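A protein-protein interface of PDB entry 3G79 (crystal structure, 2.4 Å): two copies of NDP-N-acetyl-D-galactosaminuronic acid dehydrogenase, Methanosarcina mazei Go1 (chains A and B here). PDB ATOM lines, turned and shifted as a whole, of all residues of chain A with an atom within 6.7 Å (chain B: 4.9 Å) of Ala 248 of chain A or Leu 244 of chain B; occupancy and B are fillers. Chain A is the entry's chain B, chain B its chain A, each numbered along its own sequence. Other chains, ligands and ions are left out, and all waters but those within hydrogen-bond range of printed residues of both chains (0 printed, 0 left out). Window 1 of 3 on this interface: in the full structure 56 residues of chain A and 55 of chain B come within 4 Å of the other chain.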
ATOM      1  N   ASP A 243      -2.400  16.832  25.589  1.00  0.00           N
ATOM      2  CA  ASP A 243      -3.408  15.900  25.087  1.00  0.00           C
ATOM      3  C   ASP A 243      -4.174  16.366  23.826  1.00  0.00           C
ATOM      4  O   ASP A 243      -4.372  15.604  22.880  1.00  0.00           O
ATOM      5  CB  ASP A 243      -4.404  15.628  26.179  1.00  0.00           C
ATOM      6  CG  ASP A 243      -5.232  14.448  25.891  1.00  0.00           C
ATOM      7  OD1 ASP A 243      -4.710  13.550  25.223  1.00  0.00           O
ATOM      8  OD2 ASP A 243      -6.399  14.414  26.333  1.00  0.00           O
ATOM      9  N   LEU A 244      -4.617  17.606  23.832  1.00  0.00           N
ATOM     10  CA  LEU A 244      -5.332  18.140  22.710  1.00  0.00           C
ATOM     11  C   LEU A 244      -4.434  18.331  21.486  1.00  0.00           C
ATOM     12  O   LEU A 244      -4.900  18.182  20.342  1.00  0.00           O
ATOM     13  CB  LEU A 244      -5.989  19.449  23.101  1.00  0.00           C
ATOM     14  CG  LEU A 244      -6.766  20.178  22.026  1.00  0.00           C
ATOM     15  CD1 LEU A 244      -8.108  19.597  21.852  1.00  0.00           C
ATOM     16  CD2 LEU A 244      -6.849  21.591  22.499  1.00  0.00           C
ATOM     17  N   GLN A 245      -3.156  18.646  21.715  1.00  0.00           N
ATOM     18  CA  GLN A 245      -2.200  18.717  20.633  1.00  0.00           C
ATOM     19  C   GLN A 245      -2.115  17.311  19.956  1.00  0.00           C
ATOM     20  O   GLN A 245      -2.242  17.193  18.703  1.00  0.00           O
ATOM     21  CB  GLN A 245      -0.805  19.148  21.152  1.00  0.00           C
ATOM     22  CG  GLN A 245      -0.542  20.647  21.373  1.00  0.00           C
ATOM     23  CD  GLN A 245       0.725  20.842  22.167  1.00  0.00           C
ATOM     24  OE1 GLN A 245       0.745  20.687  23.412  1.00  0.00           O
ATOM     25  NE2 GLN A 245       1.809  21.176  21.464  1.00  0.00           N
ATOM     26  N   ILE A 246      -1.927  16.259  20.775  1.00  0.00           N
ATOM     27  CA  ILE A 246      -1.870  14.918  20.241  1.00  0.00           C
ATOM     28  C   ILE A 246      -3.156  14.578  19.483  1.00  0.00           C
ATOM     29  O   ILE A 246      -3.109  14.056  18.369  1.00  0.00           O
ATOM     30  CB  ILE A 246      -1.635  13.875  21.334  1.00  0.00           C
ATOM     31  CG1 ILE A 246      -0.299  14.173  22.068  1.00  0.00           C
ATOM     32  CG2 ILE A 246      -1.699  12.468  20.715  1.00  0.00           C
ATOM     33  CD1 ILE A 246      -0.163  13.416  23.349  1.00  0.00           C
ATOM     34  N   ALA A 247      -4.296  14.889  20.069  1.00  0.00           N
ATOM     35  CA  ALA A 247      -5.578  14.581  19.419  1.00  0.00           C
ATOM     36  C   ALA A 247      -5.723  15.402  18.125  1.00  0.00           C
ATOM     37  O   ALA A 247      -6.221  14.877  17.143  1.00  0.00           O
ATOM     38  CB  ALA A 247      -6.770  14.787  20.362  1.00  0.00           C
ATOM     39  N   ALA A 248      -5.231  16.644  18.102  1.00  0.00           N
ATOM     40  CA  ALA A 248      -5.222  17.419  16.829  1.00  0.00           C
ATOM     41  C   ALA A 248      -4.527  16.696  15.662  1.00  0.00           C
ATOM     42  O   ALA A 248      -5.087  16.707  14.529  1.00  0.00           O
ATOM     43  CB  ALA A 248      -4.631  18.822  17.010  1.00  0.00           C
ATOM     44  N   ILE A 249      -3.359  16.058  15.914  1.00  0.00           N
ATOM     45  CA  ILE A 249      -2.631  15.360  14.786  1.00  0.00           C
ATOM     46  C   ILE A 249      -3.149  14.004  14.512  1.00  0.00           C
ATOM     47  O   ILE A 249      -3.120  13.581  13.370  1.00  0.00           O
ATOM     48  CB  ILE A 249      -1.079  15.161  14.888  1.00  0.00           C
ATOM     49  CG1 ILE A 249      -0.544  15.690  16.185  1.00  0.00           C
ATOM     50  CG2 ILE A 249      -0.322  15.606  13.536  1.00  0.00           C
ATOM     51  CD1 ILE A 249      -0.229  14.657  17.067  1.00  0.00           C
ATOM     52  N   ASN A 250      -3.552  13.288  15.560  1.00  0.00           N
ATOM     53  CA  ASN A 250      -4.274  12.043  15.388  1.00  0.00           C
ATOM     54  C   ASN A 250      -5.448  12.304  14.480  1.00  0.00           C
ATOM     55  O   ASN A 250      -5.665  11.580  13.519  1.00  0.00           O
ATOM     56  CB  ASN A 250      -4.694  11.468  16.723  1.00  0.00           C
ATOM     57  CG  ASN A 250      -3.532  10.776  17.468  1.00  0.00           C
ATOM     58  OD1 ASN A 250      -2.503  10.413  16.872  1.00  0.00           O
ATOM     59  ND2 ASN A 250      -3.717  10.533  18.738  1.00  0.00           N
ATOM     60  N   GLN A 251      -6.194  13.357  14.718  1.00  0.00           N
ATOM     61  CA  GLN A 251      -7.307  13.630  13.799  1.00  0.00           C
ATOM     62  C   GLN A 251      -6.842  14.018  12.402  1.00  0.00           C
ATOM     63  O   GLN A 251      -7.511  13.694  11.437  1.00  0.00           O
ATOM     64  CB  GLN A 251      -8.275  14.693  14.306  1.00  0.00           C
ATOM     65  CG  GLN A 251      -9.452  14.902  13.311  1.00  0.00           C
ATOM     66  CD  GLN A 251     -10.522  15.830  13.826  1.00  0.00           C
ATOM     67  OE1 GLN A 251     -10.591  16.110  15.028  1.00  0.00           O
ATOM     68  NE2 GLN A 251     -11.384  16.314  12.914  1.00  0.00           N
ATOM     69  N   LEU A 252      -5.715  14.703  12.287  1.00  0.00           N
ATOM     70  CA  LEU A 252      -5.196  15.059  10.958  1.00  0.00           C
ATOM     71  C   LEU A 252      -4.796  13.744  10.250  1.00  0.00           C
ATOM     72  O   LEU A 252      -5.155  13.505   9.084  1.00  0.00           O
ATOM     73  CB  LEU A 252      -4.009  16.002  11.069  1.00  0.00           C
ATOM     74  CG  LEU A 252      -3.999  17.151  10.066  1.00  0.00           C
ATOM     75  CD1 LEU A 252      -2.589  17.509   9.696  1.00  0.00           C
ATOM     76  CD2 LEU A 252      -4.817  16.870   8.842  1.00  0.00           C
ATOM     77  N   ALA A 253      -4.118  12.867  10.995  1.00  0.00           N
ATOM     78  CA  ALA A 253      -3.841  11.517  10.530  1.00  0.00           C
ATOM     79  C   ALA A 253      -5.068  10.848   9.958  1.00  0.00           C
ATOM     80  O   ALA A 253      -4.984  10.276   8.894  1.00  0.00           O
ATOM     81  CB  ALA A 253      -3.198  10.634  11.653  1.00  0.00           C
ATOM     82  N   ILE A 321     -13.933  20.649  23.726  1.00  0.00           N
ATOM     83  CA  ILE A 321     -12.818  20.154  22.926  1.00  0.00           C
ATOM     84  C   ILE A 321     -11.881  19.214  23.695  1.00  0.00           C
ATOM     85  O   ILE A 321     -11.225  18.381  23.094  1.00  0.00           O
ATOM     86  CB  ILE A 321     -11.964  21.271  22.369  1.00  0.00           C
ATOM     87  CG1 ILE A 321     -11.653  22.274  23.459  1.00  0.00           C
ATOM     88  CG2 ILE A 321     -12.675  22.003  21.259  1.00  0.00           C
ATOM     89  CD1 ILE A 321     -11.239  23.572  22.875  1.00  0.00           C
ATOM     90  N   ALA A 325     -10.943  15.631  22.592  1.00  0.00           N
ATOM     91  CA  ALA A 325      -9.547  15.191  22.535  1.00  0.00           C
ATOM     92  C   ALA A 325      -9.364  13.846  23.246  1.00  0.00           C
ATOM     93  O   ALA A 325      -8.680  12.935  22.708  1.00  0.00           O
ATOM     94  CB  ALA A 325      -8.646  16.238  23.182  1.00  0.00           C
ATOM     95  N   VAL A 328     -10.980  11.120  20.786  1.00  0.00           N
ATOM     96  CA  VAL A 328     -10.153  10.851  19.594  1.00  0.00           C
ATOM     97  C   VAL A 328      -8.918  10.097  20.036  1.00  0.00           C
ATOM     98  O   VAL A 328      -8.606   9.035  19.527  1.00  0.00           O
ATOM     99  CB  VAL A 328      -9.742  12.144  18.862  1.00  0.00           C
ATOM    100  CG1 VAL A 328      -8.567  11.899  17.936  1.00  0.00           C
ATOM    101  CG2 VAL A 328     -10.924  12.694  18.102  1.00  0.00           C
ATOM    102  N   ASN A 329      -8.239  10.609  21.028  1.00  0.00           N
ATOM    103  CA  ASN A 329      -7.096   9.878  21.544  1.00  0.00           C
ATOM    104  C   ASN A 329      -7.505   8.453  21.955  1.00  0.00           C
ATOM    105  O   ASN A 329      -6.797   7.531  21.655  1.00  0.00           O
ATOM    106  CB  ASN A 329      -6.361  10.668  22.648  1.00  0.00           C
ATOM    107  CG  ASN A 329      -5.446  11.784  22.086  1.00  0.00           C
ATOM    108  OD1 ASN A 329      -4.900  11.652  21.000  1.00  0.00           O
ATOM    109  ND2 ASN A 329      -5.287  12.887  22.825  1.00  0.00           N
ATOM    110  N   ASN B 239      -3.942  27.043   9.383  1.00  0.00           N
ATOM    111  CA  ASN B 239      -4.934  27.912   9.957  1.00  0.00           C
ATOM    112  C   ASN B 239      -5.817  27.187  10.958  1.00  0.00           C
ATOM    113  O   ASN B 239      -6.071  27.687  12.027  1.00  0.00           O
ATOM    114  CB  ASN B 239      -5.731  28.544   8.843  1.00  0.00           C
ATOM    115  CG  ASN B 239      -4.863  29.412   7.977  1.00  0.00           C
ATOM    116  OD1 ASN B 239      -4.061  30.184   8.494  1.00  0.00           O
ATOM    117  ND2 ASN B 239      -4.984  29.278   6.662  1.00  0.00           N
ATOM    118  N   THR B 240      -6.267  25.995  10.605  1.00  0.00           N
ATOM    119  CA  THR B 240      -7.016  25.134  11.509  1.00  0.00           C
ATOM    120  C   THR B 240      -6.317  24.903  12.901  1.00  0.00           C
ATOM    121  O   THR B 240      -6.915  25.108  13.975  1.00  0.00           O
ATOM    122  CB  THR B 240      -7.325  23.817  10.749  1.00  0.00           C
ATOM    123  OG1 THR B 240      -8.295  24.101   9.721  1.00  0.00           O
ATOM    124  CG2 THR B 240      -7.862  22.720  11.689  1.00  0.00           C
ATOM    125  N   PHE B 241      -5.043  24.517  12.873  1.00  0.00           N
ATOM    126  CA  PHE B 241      -4.317  24.212  14.097  1.00  0.00           C
ATOM    127  C   PHE B 241      -4.151  25.466  14.935  1.00  0.00           C
ATOM    128  O   PHE B 241      -4.321  25.411  16.147  1.00  0.00           O
ATOM    129  CB  PHE B 241      -2.978  23.529  13.767  1.00  0.00           C
ATOM    130  CG  PHE B 241      -3.102  22.054  13.620  1.00  0.00           C
ATOM    131  CD1 PHE B 241      -4.125  21.500  12.864  1.00  0.00           C
ATOM    132  CD2 PHE B 241      -2.237  21.204  14.278  1.00  0.00           C
ATOM    133  CE1 PHE B 241      -4.259  20.128  12.746  1.00  0.00           C
ATOM    134  CE2 PHE B 241      -2.377  19.828  14.176  1.00  0.00           C
ATOM    135  CZ  PHE B 241      -3.371  19.291  13.404  1.00  0.00           C
ATOM    136  N   ARG B 242      -3.874  26.597  14.277  1.00  0.00           N
ATOM    137  CA  ARG B 242      -3.824  27.906  14.951  1.00  0.00           C
ATOM    138  C   ARG B 242      -5.181  28.215  15.563  1.00  0.00           C
ATOM    139  O   ARG B 242      -5.257  28.532  16.741  1.00  0.00           O
ATOM    140  CB  ARG B 242      -3.348  29.088  14.035  1.00  0.00           C
ATOM    141  CG  ARG B 242      -3.680  30.489  14.626  1.00  0.00           C
ATOM    142  CD  ARG B 242      -2.822  31.674  14.130  1.00  0.00           C
ATOM    143  NE  ARG B 242      -1.596  31.726  14.908  1.00  0.00           N
ATOM    144  CZ  ARG B 242      -1.152  32.770  15.605  1.00  0.00           C
ATOM    145  NH1 ARG B 242      -1.799  33.941  15.599  1.00  0.00           N
ATOM    146  NH2 ARG B 242      -0.031  32.625  16.298  1.00  0.00           N
ATOM    147  N   ASP B 243      -6.238  28.079  14.765  1.00  0.00           N
ATOM    148  CA  ASP B 243      -7.593  28.320  15.211  1.00  0.00           C
ATOM    149  C   ASP B 243      -7.919  27.481  16.429  1.00  0.00           C
ATOM    150  O   ASP B 243      -8.487  27.951  17.396  1.00  0.00           O
ATOM    151  CB  ASP B 243      -8.583  28.067  14.072  1.00  0.00           C
ATOM    152  CG  ASP B 243      -9.998  28.428  14.446  1.00  0.00           C
ATOM    153  OD1 ASP B 243     -10.203  29.437  15.147  1.00  0.00           O
ATOM    154  OD2 ASP B 243     -10.925  27.707  14.050  1.00  0.00           O
ATOM    155  N   LEU B 244      -7.525  26.233  16.398  1.00  0.00           N
ATOM    156  CA  LEU B 244      -7.651  25.366  17.562  1.00  0.00           C
ATOM    157  C   LEU B 244      -6.827  25.814  18.773  1.00  0.00           C
ATOM    158  O   LEU B 244      -7.332  25.727  19.905  1.00  0.00           O
ATOM    159  CB  LEU B 244      -7.334  23.916  17.186  1.00  0.00           C
ATOM    160  CG  LEU B 244      -7.273  22.955  18.377  1.00  0.00           C
ATOM    161  CD1 LEU B 244      -8.663  22.751  19.030  1.00  0.00           C
ATOM    162  CD2 LEU B 244      -6.703  21.641  17.954  1.00  0.00           C
ATOM    163  N   GLN B 245      -5.595  26.304  18.574  1.00  0.00           N
ATOM    164  CA  GLN B 245      -4.844  26.760  19.761  1.00  0.00           C
ATOM    165  C   GLN B 245      -5.517  27.942  20.426  1.00  0.00           C
ATOM    166  O   GLN B 245      -5.426  28.149  21.657  1.00  0.00           O
ATOM    167  CB  GLN B 245      -3.311  26.953  19.587  1.00  0.00           C
ATOM    168  CG  GLN B 245      -2.829  27.549  18.318  1.00  0.00           C
ATOM    169  CD  GLN B 245      -1.314  27.313  17.967  1.00  0.00           C
ATOM    170  OE1 GLN B 245      -0.975  27.239  16.762  1.00  0.00           O
ATOM    171  NE2 GLN B 245      -0.431  27.219  18.982  1.00  0.00           N
ATOM    172  N   ILE B 246      -6.248  28.702  19.618  1.00  0.00           N
ATOM    173  CA  ILE B 246      -6.908  29.878  20.127  1.00  0.00           C
ATOM    174  C   ILE B 246      -8.156  29.439  20.848  1.00  0.00           C
ATOM    175  O   ILE B 246      -8.526  29.985  21.881  1.00  0.00           O
ATOM    176  CB  ILE B 246      -7.250  30.830  18.998  1.00  0.00           C
ATOM    177  CG1 ILE B 246      -6.009  31.621  18.574  1.00  0.00           C
ATOM    178  CG2 ILE B 246      -8.446  31.805  19.398  1.00  0.00           C
ATOM    179  CD1 ILE B 246      -6.217  32.312  17.194  1.00  0.00           C
ATOM    180  N   ALA B 247      -8.841  28.465  20.293  1.00  0.00           N
ATOM    181  CA  ALA B 247     -10.037  28.036  20.933  1.00  0.00           C
ATOM    182  C   ALA B 247      -9.660  27.380  22.259  1.00  0.00           C
ATOM    183  O   ALA B 247     -10.373  27.585  23.240  1.00  0.00           O
ATOM    184  CB  ALA B 247     -10.860  27.130  20.048  1.00  0.00           C
ATOM    185  N   ALA B 248      -8.506  26.698  22.294  1.00  0.00           N
ATOM    186  CA  ALA B 248      -7.932  26.131  23.542  1.00  0.00           C
ATOM    187  C   ALA B 248      -7.789  27.083  24.704  1.00  0.00           C
ATOM    188  O   ALA B 248      -8.268  26.728  25.809  1.00  0.00           O
ATOM    189  CB  ALA B 248      -6.579  25.442  23.304  1.00  0.00           C
ATOM    190  N   ILE B 321     -12.927  17.807  16.153  1.00  0.00           N
ATOM    191  CA  ILE B 321     -12.282  18.791  17.011  1.00  0.00           C
ATOM    192  C   ILE B 321     -12.234  20.172  16.363  1.00  0.00           C
ATOM    193  O   ILE B 321     -12.374  21.178  17.039  1.00  0.00           O
ATOM    194  CB  ILE B 321     -10.852  18.355  17.384  1.00  0.00           C
ATOM    195  CG1 ILE B 321     -10.919  17.157  18.322  1.00  0.00           C
ATOM    196  CG2 ILE B 321     -10.129  19.461  18.080  1.00  0.00           C
ATOM    197  CD1 ILE B 321      -9.645  16.413  18.375  1.00  0.00           C
ATOM    198  N   TYR B 322     -12.037  20.246  15.068  1.00  0.00           N
ATOM    199  CA  TYR B 322     -11.801  21.579  14.496  1.00  0.00           C
ATOM    200  C   TYR B 322     -13.119  22.302  14.444  1.00  0.00           C
ATOM    201  O   TYR B 322     -13.188  23.488  14.745  1.00  0.00           O
ATOM    202  CB  TYR B 322     -11.161  21.498  13.108  1.00  0.00           C
ATOM    203  CG  TYR B 322     -10.068  20.462  13.009  1.00  0.00           C
ATOM    204  CD1 TYR B 322      -8.999  20.427  13.941  1.00  0.00           C
ATOM    205  CD2 TYR B 322     -10.070  19.539  11.976  1.00  0.00           C
ATOM    206  CE1 TYR B 322      -7.960  19.479  13.840  1.00  0.00           C
ATOM    207  CE2 TYR B 322      -9.042  18.584  11.863  1.00  0.00           C
ATOM    208  CZ  TYR B 322      -7.991  18.560  12.797  1.00  0.00           C
ATOM    209  OH  TYR B 322      -7.000  17.610  12.639  1.00  0.00           O
ATOM    210  N   ALA B 325     -13.680  23.715  17.630  1.00  0.00           N
ATOM    211  CA  ALA B 325     -12.870  24.947  17.760  1.00  0.00           C
ATOM    212  C   ALA B 325     -13.559  26.190  17.152  1.00  0.00           C
ATOM    213  O   ALA B 325     -13.572  27.280  17.758  1.00  0.00           O
ATOM    214  CB  ALA B 325     -11.524  24.773  17.143  1.00  0.00           C
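Printed residues of chain B that touch a printed residue of chain A: Phe 241, Leu 244, Ala 248, Ile 321 and Tyr 322. Hydrophobic or aromatic side chains of chain A within 4 Å of the printed part of chain B: Leu 244, Ala 247, Ala 248, Leu 252 and Val 328. Among the printed residues, no Asp or Glu carboxylate lies within 4 Å of a Lys or Arg side-chain nitrogen of the other chain.
The backbone NH (N) of Ala 247 of chain A lies close to the side-chain amide oxygen (OD1) of Asn 329 of chain A (3.4 Å).
Ala 248 of chain A touches three residues of chain B. Leu 244 of chain B touches just one residue of chain A: Ala 248 (3.6 Å). Printed residues of chain B within 4 Å of Leu 244 of chain A: Ala 248. Of the printed residues of chain B, Ala 247 of chain A touches Ile 321. Printed residues of chain B within 4 Å of Leu 252 of chain A: Tyr 322 (3.2 Å). Thr 240 of chain B touches none of the printed residues of chain A. Ile 321 of chain A touches none of the printed residues of chain B. The nearest printed residue of chain B that does not touch Val 328 of chain A is Tyr 322 of chain B (7.9 Å).
The side-chain hydroxyl (OH) of Tyr 322 of chain B is in hydrogen-bond range of the backbone carbonyl oxygen (O) of Ala 248 of chain A. The backbone NH (N) of Ile 321 of chain B lies within hydrogen-bond range of the side-chain amide oxygen (OE1) of Gln 251 of chain A (3.1 Å). The side-chain hydroxyl (OH) of Tyr 322 of chain B lies within hydrogen-bond range of the backbone NH (N) of Leu 252 of chain A.
Leu 244 of chain A touches Ala 248 of chain B, and with the chains exchanged Ala 248 of chain A touches Leu 244 of chain B. Ala 247 of chain A touches Ile 321 of chain B, but with the chains exchanged Ile 321 of chain A does not touch Ala 247 of chain B (4.1 Å). 8 positions are printed for both chains.
Among the printed residues, merely in contact across the chains: Leu 244 of chain A with Ala 248 of chain B, Ala 247 of chain A with Ile 321 of chain B, Ala 248 of chain A with Phe 241 of chain B, Ala 248 of chain A with Leu 244 of chain B, Gln 251 of chain A with Tyr 322 of chain B and Val 328 of chain A with Ile 321 of chain B.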
